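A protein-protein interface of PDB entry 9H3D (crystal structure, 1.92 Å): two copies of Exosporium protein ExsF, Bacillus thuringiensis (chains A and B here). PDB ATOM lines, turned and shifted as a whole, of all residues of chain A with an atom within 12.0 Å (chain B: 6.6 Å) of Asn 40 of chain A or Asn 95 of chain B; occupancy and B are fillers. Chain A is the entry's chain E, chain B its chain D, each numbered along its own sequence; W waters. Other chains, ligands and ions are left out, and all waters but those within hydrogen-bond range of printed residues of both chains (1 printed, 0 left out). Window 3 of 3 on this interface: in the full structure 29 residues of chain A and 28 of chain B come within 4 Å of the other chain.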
ATOM      1  N   PHE A  16      -9.382  24.475 -19.617  1.00  0.00           N
ATOM      2  CA  PHE A  16      -7.947  24.225 -19.632  1.00  0.00           C
ATOM      3  C   PHE A  16      -7.446  24.189 -21.067  1.00  0.00           C
ATOM      4  O   PHE A  16      -8.223  24.097 -22.021  1.00  0.00           O
ATOM      5  CB  PHE A  16      -7.583  22.914 -18.916  1.00  0.00           C
ATOM      6  CG  PHE A  16      -8.171  21.671 -19.552  1.00  0.00           C
ATOM      7  CD1 PHE A  16      -9.490  21.317 -19.321  1.00  0.00           C
ATOM      8  CD2 PHE A  16      -7.397  20.859 -20.366  1.00  0.00           C
ATOM      9  CE1 PHE A  16     -10.028  20.168 -19.885  1.00  0.00           C
ATOM     10  CE2 PHE A  16      -7.929  19.718 -20.946  1.00  0.00           C
ATOM     11  CZ  PHE A  16      -9.251  19.373 -20.699  1.00  0.00           C
ATOM     12  N   VAL A  35     -13.121  21.787 -21.799  1.00  0.00           N
ATOM     13  CA  VAL A  35     -13.841  21.764 -20.527  1.00  0.00           C
ATOM     14  C   VAL A  35     -14.179  20.334 -20.095  1.00  0.00           C
ATOM     15  O   VAL A  35     -14.914  20.137 -19.122  1.00  0.00           O
ATOM     16  CB  VAL A  35     -15.122  22.623 -20.594  1.00  0.00           C
ATOM     17  CG1 VAL A  35     -14.785  24.085 -20.839  1.00  0.00           C
ATOM     18  CG2 VAL A  35     -16.044  22.112 -21.683  1.00  0.00           C
ATOM     19  N   SER A  36     -13.614  19.325 -20.767  1.00  0.00           N
ATOM     20  CA  SER A  36     -13.946  17.921 -20.509  1.00  0.00           C
ATOM     21  C   SER A  36     -12.711  17.120 -20.120  1.00  0.00           C
ATOM     22  O   SER A  36     -12.099  16.472 -20.979  1.00  0.00           O
ATOM     23  CB  SER A  36     -14.602  17.290 -21.737  1.00  0.00           C
ATOM     24  OG  SER A  36     -15.740  18.029 -22.111  1.00  0.00           O
ATOM     25  N   PRO A  37     -12.336  17.093 -18.833  1.00  0.00           N
ATOM     26  CA  PRO A  37     -11.113  16.373 -18.440  1.00  0.00           C
ATOM     27  C   PRO A  37     -11.253  14.864 -18.304  1.00  0.00           C
ATOM     28  O   PRO A  37     -10.219  14.179 -18.336  1.00  0.00           O
ATOM     29  CB  PRO A  37     -10.769  16.996 -17.082  1.00  0.00           C
ATOM     30  CG  PRO A  37     -12.130  17.313 -16.521  1.00  0.00           C
ATOM     31  CD  PRO A  37     -12.904  17.846 -17.702  1.00  0.00           C
ATOM     32  N   ASN A  38     -12.451  14.322 -18.109  1.00  0.00           N
ATOM     33  CA  ASN A  38     -12.554  12.867 -17.938  1.00  0.00           C
ATOM     34  C   ASN A  38     -12.267  12.166 -19.258  1.00  0.00           C
ATOM     35  O   ASN A  38     -13.056  12.305 -20.201  1.00  0.00           O
ATOM     36  CB  ASN A  38     -13.935  12.465 -17.422  1.00  0.00           C
ATOM     37  CG  ASN A  38     -14.006  11.006 -16.989  1.00  0.00           C
ATOM     38  OD1 ASN A  38     -13.610  10.093 -17.726  1.00  0.00           O
ATOM     39  ND2 ASN A  38     -14.507  10.780 -15.771  1.00  0.00           N
ATOM     40  N   PRO A  39     -11.192  11.385 -19.367  1.00  0.00           N
ATOM     41  CA  PRO A  39     -10.878  10.751 -20.656  1.00  0.00           C
ATOM     42  C   PRO A  39     -11.828   9.621 -21.031  1.00  0.00           C
ATOM     43  O   PRO A  39     -11.934   9.301 -22.221  1.00  0.00           O
ATOM     44  CB  PRO A  39      -9.460  10.224 -20.439  1.00  0.00           C
ATOM     45  CG  PRO A  39      -9.459   9.868 -18.990  1.00  0.00           C
ATOM     46  CD  PRO A  39     -10.290  10.922 -18.300  1.00  0.00           C
ATOM     47  N   ASN A  40     -12.520   9.006 -20.070  1.00  0.00           N
ATOM     48  CA  ASN A  40     -13.371   7.859 -20.386  1.00  0.00           C
ATOM     49  C   ASN A  40     -14.824   8.254 -20.624  1.00  0.00           C
ATOM     50  O   ASN A  40     -15.487   7.698 -21.508  1.00  0.00           O
ATOM     51  CB  ASN A  40     -13.307   6.832 -19.261  1.00  0.00           C
ATOM     52  CG  ASN A  40     -11.895   6.394 -18.954  1.00  0.00           C
ATOM     53  OD1 ASN A  40     -11.020   6.392 -19.824  1.00  0.00           O
ATOM     54  ND2 ASN A  40     -11.668   6.011 -17.714  1.00  0.00           N
ATOM     55  N   ILE A  41     -15.340   9.184 -19.833  1.00  0.00           N
ATOM     56  CA  ILE A  41     -16.718   9.644 -19.959  1.00  0.00           C
ATOM     57  C   ILE A  41     -16.655  11.160 -20.089  1.00  0.00           C
ATOM     58  O   ILE A  41     -16.837  11.879 -19.098  1.00  0.00           O
ATOM     59  CB  ILE A  41     -17.565   9.193 -18.760  1.00  0.00           C
ATOM     60  CG1 ILE A  41     -17.462   7.664 -18.585  1.00  0.00           C
ATOM     61  CG2 ILE A  41     -19.018   9.611 -18.942  1.00  0.00           C
ATOM     62  CD1 ILE A  41     -18.023   7.162 -17.257  1.00  0.00           C
ATOM     63  N   PRO A  42     -16.332  11.676 -21.273  1.00  0.00           N
ATOM     64  CA  PRO A  42     -16.144  13.124 -21.447  1.00  0.00           C
ATOM     65  C   PRO A  42     -17.456  13.873 -21.281  1.00  0.00           C
ATOM     66  O   PRO A  42     -18.428  13.606 -21.996  1.00  0.00           O
ATOM     67  CB  PRO A  42     -15.614  13.242 -22.882  1.00  0.00           C
ATOM     68  CG  PRO A  42     -15.179  11.859 -23.264  1.00  0.00           C
ATOM     69  CD  PRO A  42     -16.036  10.919 -22.498  1.00  0.00           C
ATOM     70  N   VAL A  43     -17.486  14.801 -20.325  1.00  0.00           N
ATOM     71  CA  VAL A  43     -18.599  15.745 -20.206  1.00  0.00           C
ATOM     72  C   VAL A  43     -18.054  17.130 -19.886  1.00  0.00           C
ATOM     73  O   VAL A  43     -17.015  17.289 -19.235  1.00  0.00           O
ATOM     74  CB  VAL A  43     -19.621  15.318 -19.107  1.00  0.00           C
ATOM     75  CG1 VAL A  43     -20.257  13.977 -19.436  1.00  0.00           C
ATOM     76  CG2 VAL A  43     -18.968  15.244 -17.758  1.00  0.00           C
ATOM     77  N   PRO A  44     -18.754  18.164 -20.355  1.00  0.00           N
ATOM     78  CA  PRO A  44     -18.342  19.541 -20.014  1.00  0.00           C
ATOM     79  C   PRO A  44     -18.504  19.773 -18.519  1.00  0.00           C
ATOM     80  O   PRO A  44     -19.602  19.653 -17.978  1.00  0.00           O
ATOM     81  CB  PRO A  44     -19.297  20.410 -20.835  1.00  0.00           C
ATOM     82  CG  PRO A  44     -20.534  19.519 -21.017  1.00  0.00           C
ATOM     83  CD  PRO A  44     -19.985  18.132 -21.174  1.00  0.00           C
ATOM     84  N   VAL A  45     -17.399  20.069 -17.832  1.00  0.00           N
ATOM     85  CA  VAL A  45     -17.514  20.287 -16.395  1.00  0.00           C
ATOM     86  C   VAL A  45     -17.840  21.764 -16.206  1.00  0.00           C
ATOM     87  O   VAL A  45     -16.983  22.584 -15.834  1.00  0.00           O
ATOM     88  CB  VAL A  45     -16.254  19.825 -15.635  1.00  0.00           C
ATOM     89  CG1 VAL A  45     -16.451  19.987 -14.139  1.00  0.00           C
ATOM     90  CG2 VAL A  45     -16.003  18.358 -15.941  1.00  0.00           C
ATOM     91  N   PHE B  27       5.178   5.948 -14.974  1.00  0.00           N
ATOM     92  CA  PHE B  27       3.815   5.437 -14.820  1.00  0.00           C
ATOM     93  C   PHE B  27       3.622   4.608 -13.553  1.00  0.00           C
ATOM     94  O   PHE B  27       2.720   3.773 -13.486  1.00  0.00           O
ATOM     95  CB  PHE B  27       3.384   4.643 -16.057  1.00  0.00           C
ATOM     96  CG  PHE B  27       3.084   5.516 -17.237  1.00  0.00           C
ATOM     97  CD1 PHE B  27       1.898   6.240 -17.292  1.00  0.00           C
ATOM     98  CD2 PHE B  27       3.985   5.628 -18.281  1.00  0.00           C
ATOM     99  CE1 PHE B  27       1.613   7.069 -18.375  1.00  0.00           C
ATOM    100  CE2 PHE B  27       3.706   6.452 -19.368  1.00  0.00           C
ATOM    101  CZ  PHE B  27       2.523   7.172 -19.416  1.00  0.00           C
ATOM    102  N   LEU B  88      -2.470  13.348 -13.142  1.00  0.00           N
ATOM    103  CA  LEU B  88      -3.346  12.441 -12.424  1.00  0.00           C
ATOM    104  C   LEU B  88      -3.872  11.385 -13.388  1.00  0.00           C
ATOM    105  O   LEU B  88      -4.150  11.679 -14.551  1.00  0.00           O
ATOM    106  CB  LEU B  88      -4.516  13.188 -11.799  1.00  0.00           C
ATOM    107  CG  LEU B  88      -4.126  14.091 -10.647  1.00  0.00           C
ATOM    108  CD1 LEU B  88      -5.361  14.888 -10.237  1.00  0.00           C
ATOM    109  CD2 LEU B  88      -3.604  13.244  -9.499  1.00  0.00           C
ATOM    110  N   SER B  89      -3.992  10.155 -12.906  1.00  0.00           N
ATOM    111  CA  SER B  89      -4.554   9.079 -13.704  1.00  0.00           C
ATOM    112  C   SER B  89      -5.875   8.614 -13.102  1.00  0.00           C
ATOM    113  O   SER B  89      -6.150   8.785 -11.910  1.00  0.00           O
ATOM    114  CB  SER B  89      -3.566   7.902 -13.836  1.00  0.00           C
ATOM    115  OG  SER B  89      -3.250   7.322 -12.577  1.00  0.00           O
ATOM    116  N   LEU B  90      -6.701   8.032 -13.962  1.00  0.00           N
ATOM    117  CA  LEU B  90      -8.035   7.568 -13.608  1.00  0.00           C
ATOM    118  C   LEU B  90      -8.069   6.061 -13.852  1.00  0.00           C
ATOM    119  O   LEU B  90      -7.985   5.610 -15.001  1.00  0.00           O
ATOM    120  CB  LEU B  90      -9.092   8.303 -14.439  1.00  0.00           C
ATOM    121  CG  LEU B  90     -10.533   8.451 -13.935  1.00  0.00           C
ATOM    122  CD1 LEU B  90     -11.406   9.047 -15.017  1.00  0.00           C
ATOM    123  CD2 LEU B  90     -11.073   7.111 -13.504  1.00  0.00           C
ATOM    124  N   GLY B  91      -8.190   5.283 -12.784  1.00  0.00           N
ATOM    125  CA  GLY B  91      -8.271   3.843 -12.957  1.00  0.00           C
ATOM    126  C   GLY B  91      -6.918   3.170 -13.081  1.00  0.00           C
ATOM    127  O   GLY B  91      -6.534   2.391 -12.199  1.00  0.00           O
ATOM    128  N   THR B  92      -6.190   3.431 -14.164  1.00  0.00           N
ATOM    129  CA  THR B  92      -4.850   2.891 -14.324  1.00  0.00           C
ATOM    130  C   THR B  92      -3.881   4.006 -14.680  1.00  0.00           C
ATOM    131  O   THR B  92      -4.287   5.031 -15.244  1.00  0.00           O
ATOM    132  CB  THR B  92      -4.778   1.814 -15.417  1.00  0.00           C
ATOM    133  OG1 THR B  92      -5.582   2.217 -16.533  1.00  0.00           O
ATOM    134  CG2 THR B  92      -5.219   0.465 -14.878  1.00  0.00           C
ATOM    135  N   PRO B  93      -2.583   3.816 -14.388  1.00  0.00           N
ATOM    136  CA  PRO B  93      -1.602   4.884 -14.642  1.00  0.00           C
ATOM    137  C   PRO B  93      -1.594   5.402 -16.067  1.00  0.00           C
ATOM    138  O   PRO B  93      -1.339   6.592 -16.278  1.00  0.00           O
ATOM    139  CB  PRO B  93      -0.261   4.217 -14.288  1.00  0.00           C
ATOM    140  CG  PRO B  93      -0.617   3.172 -13.283  1.00  0.00           C
ATOM    141  CD  PRO B  93      -1.988   2.676 -13.662  1.00  0.00           C
ATOM    142  N   ALA B  94      -1.861   4.565 -17.063  1.00  0.00           N
ATOM    143  CA  ALA B  94      -1.785   5.081 -18.422  1.00  0.00           C
ATOM    144  C   ALA B  94      -2.963   5.984 -18.756  1.00  0.00           C
ATOM    145  O   ALA B  94      -2.875   6.768 -19.708  1.00  0.00           O
ATOM    146  CB  ALA B  94      -1.699   3.931 -19.425  1.00  0.00           C
ATOM    147  N   ASN B  95      -4.050   5.914 -17.985  1.00  0.00           N
ATOM    148  CA  ASN B  95      -5.294   6.613 -18.334  1.00  0.00           C
ATOM    149  C   ASN B  95      -5.309   8.001 -17.683  1.00  0.00           C
ATOM    150  O   ASN B  95      -6.018   8.268 -16.706  1.00  0.00           O
ATOM    151  CB  ASN B  95      -6.492   5.773 -17.914  1.00  0.00           C
ATOM    152  CG  ASN B  95      -7.788   6.277 -18.478  1.00  0.00           C
ATOM    153  OD1 ASN B  95      -8.815   6.246 -17.804  1.00  0.00           O
ATOM    154  ND2 ASN B  95      -7.757   6.745 -19.726  1.00  0.00           N
ATOM    155  N   ILE B  96      -4.497   8.902 -18.254  1.00  0.00           N
ATOM    156  CA  ILE B  96      -4.223  10.183 -17.613  1.00  0.00           C
ATOM    157  C   ILE B  96      -5.293  11.205 -17.973  1.00  0.00           C
ATOM    158  O   ILE B  96      -5.946  11.134 -19.019  1.00  0.00           O
ATOM    159  CB  ILE B  96      -2.815  10.709 -17.961  1.00  0.00           C
ATOM    160  CG1 ILE B  96      -2.676  10.933 -19.460  1.00  0.00           C
ATOM    161  CG2 ILE B  96      -1.729   9.757 -17.445  1.00  0.00           C
ATOM    162  CD1 ILE B  96      -1.335  11.458 -19.841  1.00  0.00           C
ATOM    163  N   ILE B  97      -5.454  12.179 -17.084  1.00  0.00           N
ATOM    164  CA  ILE B  97      -6.548  13.142 -17.128  1.00  0.00           C
ATOM    165  C   ILE B  97      -6.020  14.426 -17.768  1.00  0.00           C
ATOM    166  O   ILE B  97      -5.206  15.132 -17.143  1.00  0.00           O
ATOM    167  CB  ILE B  97      -7.112  13.405 -15.727  1.00  0.00           C
ATOM    168  CG1 ILE B  97      -7.686  12.109 -15.133  1.00  0.00           C
ATOM    169  CG2 ILE B  97      -8.112  14.527 -15.757  1.00  0.00           C
ATOM    170  CD1 ILE B  97      -7.915  12.146 -13.615  1.00  0.00           C
ATOM    171  N   ASP B 129     -13.365   4.434  -9.291  1.00  0.00           N
ATOM    172  CA  ASP B 129     -12.303   5.229  -9.896  1.00  0.00           C
ATOM    173  C   ASP B 129     -11.165   5.403  -8.899  1.00  0.00           C
ATOM    174  O   ASP B 129     -11.372   5.849  -7.764  1.00  0.00           O
ATOM    175  CB  ASP B 129     -12.821   6.604 -10.331  1.00  0.00           C
ATOM    176  CG  ASP B 129     -13.698   6.542 -11.587  1.00  0.00           C
ATOM    177  OD1 ASP B 129     -13.772   5.465 -12.219  1.00  0.00           O
ATOM    178  OD2 ASP B 129     -14.308   7.573 -11.949  1.00  0.00           O
HETATM  179  O   HOH W   1     -15.374   7.961 -14.227  1.00  0.00           O
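No position is printed for both chains. Of the 6 pairs that touch across the chains among the printed residues, none has its exchanged pair printed and touching as well.
The backbone carbonyl oxygen (O) of Leu 88 of chain B is in hydrogen-bond range of the backbone NH (N) of Ile 97 of chain B, 2.9 Å away. The backbone carbonyl oxygen (O) of Asn 95 of chain B is in hydrogen-bond range of the backbone NH (N) of Leu 90 of chain B (2.8 Å). The side-chain amide oxygen (OD1) of Asn 38 of chain A is in hydrogen-bond range of the backbone NH (N) of Asn 40 of chain A (2.8 Å). The side-chain amide oxygen (OD1) of Asn 38 of chain A lies within hydrogen-bond range of the backbone NH (N) of Ile 41 of chain A.
Val 35 of chain A touches none of the printed residues of chain B. Of the printed residues of chain B, Pro 37 of chain A touches Ile 97 (3.3 Å). Printed residues of chain B within 4 Å of Asn 38 of chain A: Leu 90. Of the printed residues of chain B, Pro 39 of chain A touches Leu 90, Asn 95 and Ile 96. Asn 40 of chain A touches one residue of chain B. Pro 44 of chain A touches none of the printed residues of chain B. Of chain A, only Asn 38 and Pro 39 come within 4 Å of Leu 90 of chain B. No residue of chain A comes within 4 Å of Gly 91 of chain B. No residue of chain A comes within 4 Å of Pro 93 of chain B. No residue of chain A comes within 4 Å of Ala 94 of chain B. Asn 95 of chain B touches just these residues of chain A: Pro 39 (3.6 Å) and Asn 40 (2.9 Å). Of the printed residues of chain A, Ile 96 of chain B touches Pro 39. Ile 97 of chain B touches one residue of chain A. The nearest residue of chain B that does not touch Asn 40 of chain A is Leu 90 of chain B (4.1 Å).
Water W1 bridges OD2 of Asp 129 of chain B (2.5 Å) and ND2 of Asn 38 of chain A (3.3 Å).
Among the printed residues, pairs that only touch across the chains: Pro 37 of chain A with Ile 97 of chain B (3.3 Å), Asn 38 of chain A with Leu 90 of chain B (3.6 Å), Pro 39 of chain A with Asn 95 of chain B (3.6 Å), Pro 39 of chain A with Ile 96 of chain B (3.7 Å) and Pro 39 of chain A with Leu 90 of chain B (3.9 Å).
The side-chain amide oxygen (OD1) of Asn 95 of chain B sits at hydrogen-bond distance from the side-chain amide nitrogen (ND2) of Asn 40 of chain A (2.9 Å).
Hydrophobic or aromatic side chains of chain B that line the printed part of chain A: Leu 90 and Ile 97. Hydrophobic or aromatic side chains of chain A that line the printed part of chain B: Pro 37 and Pro 39. Among the printed residues, 6 pairs touch across the chains.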
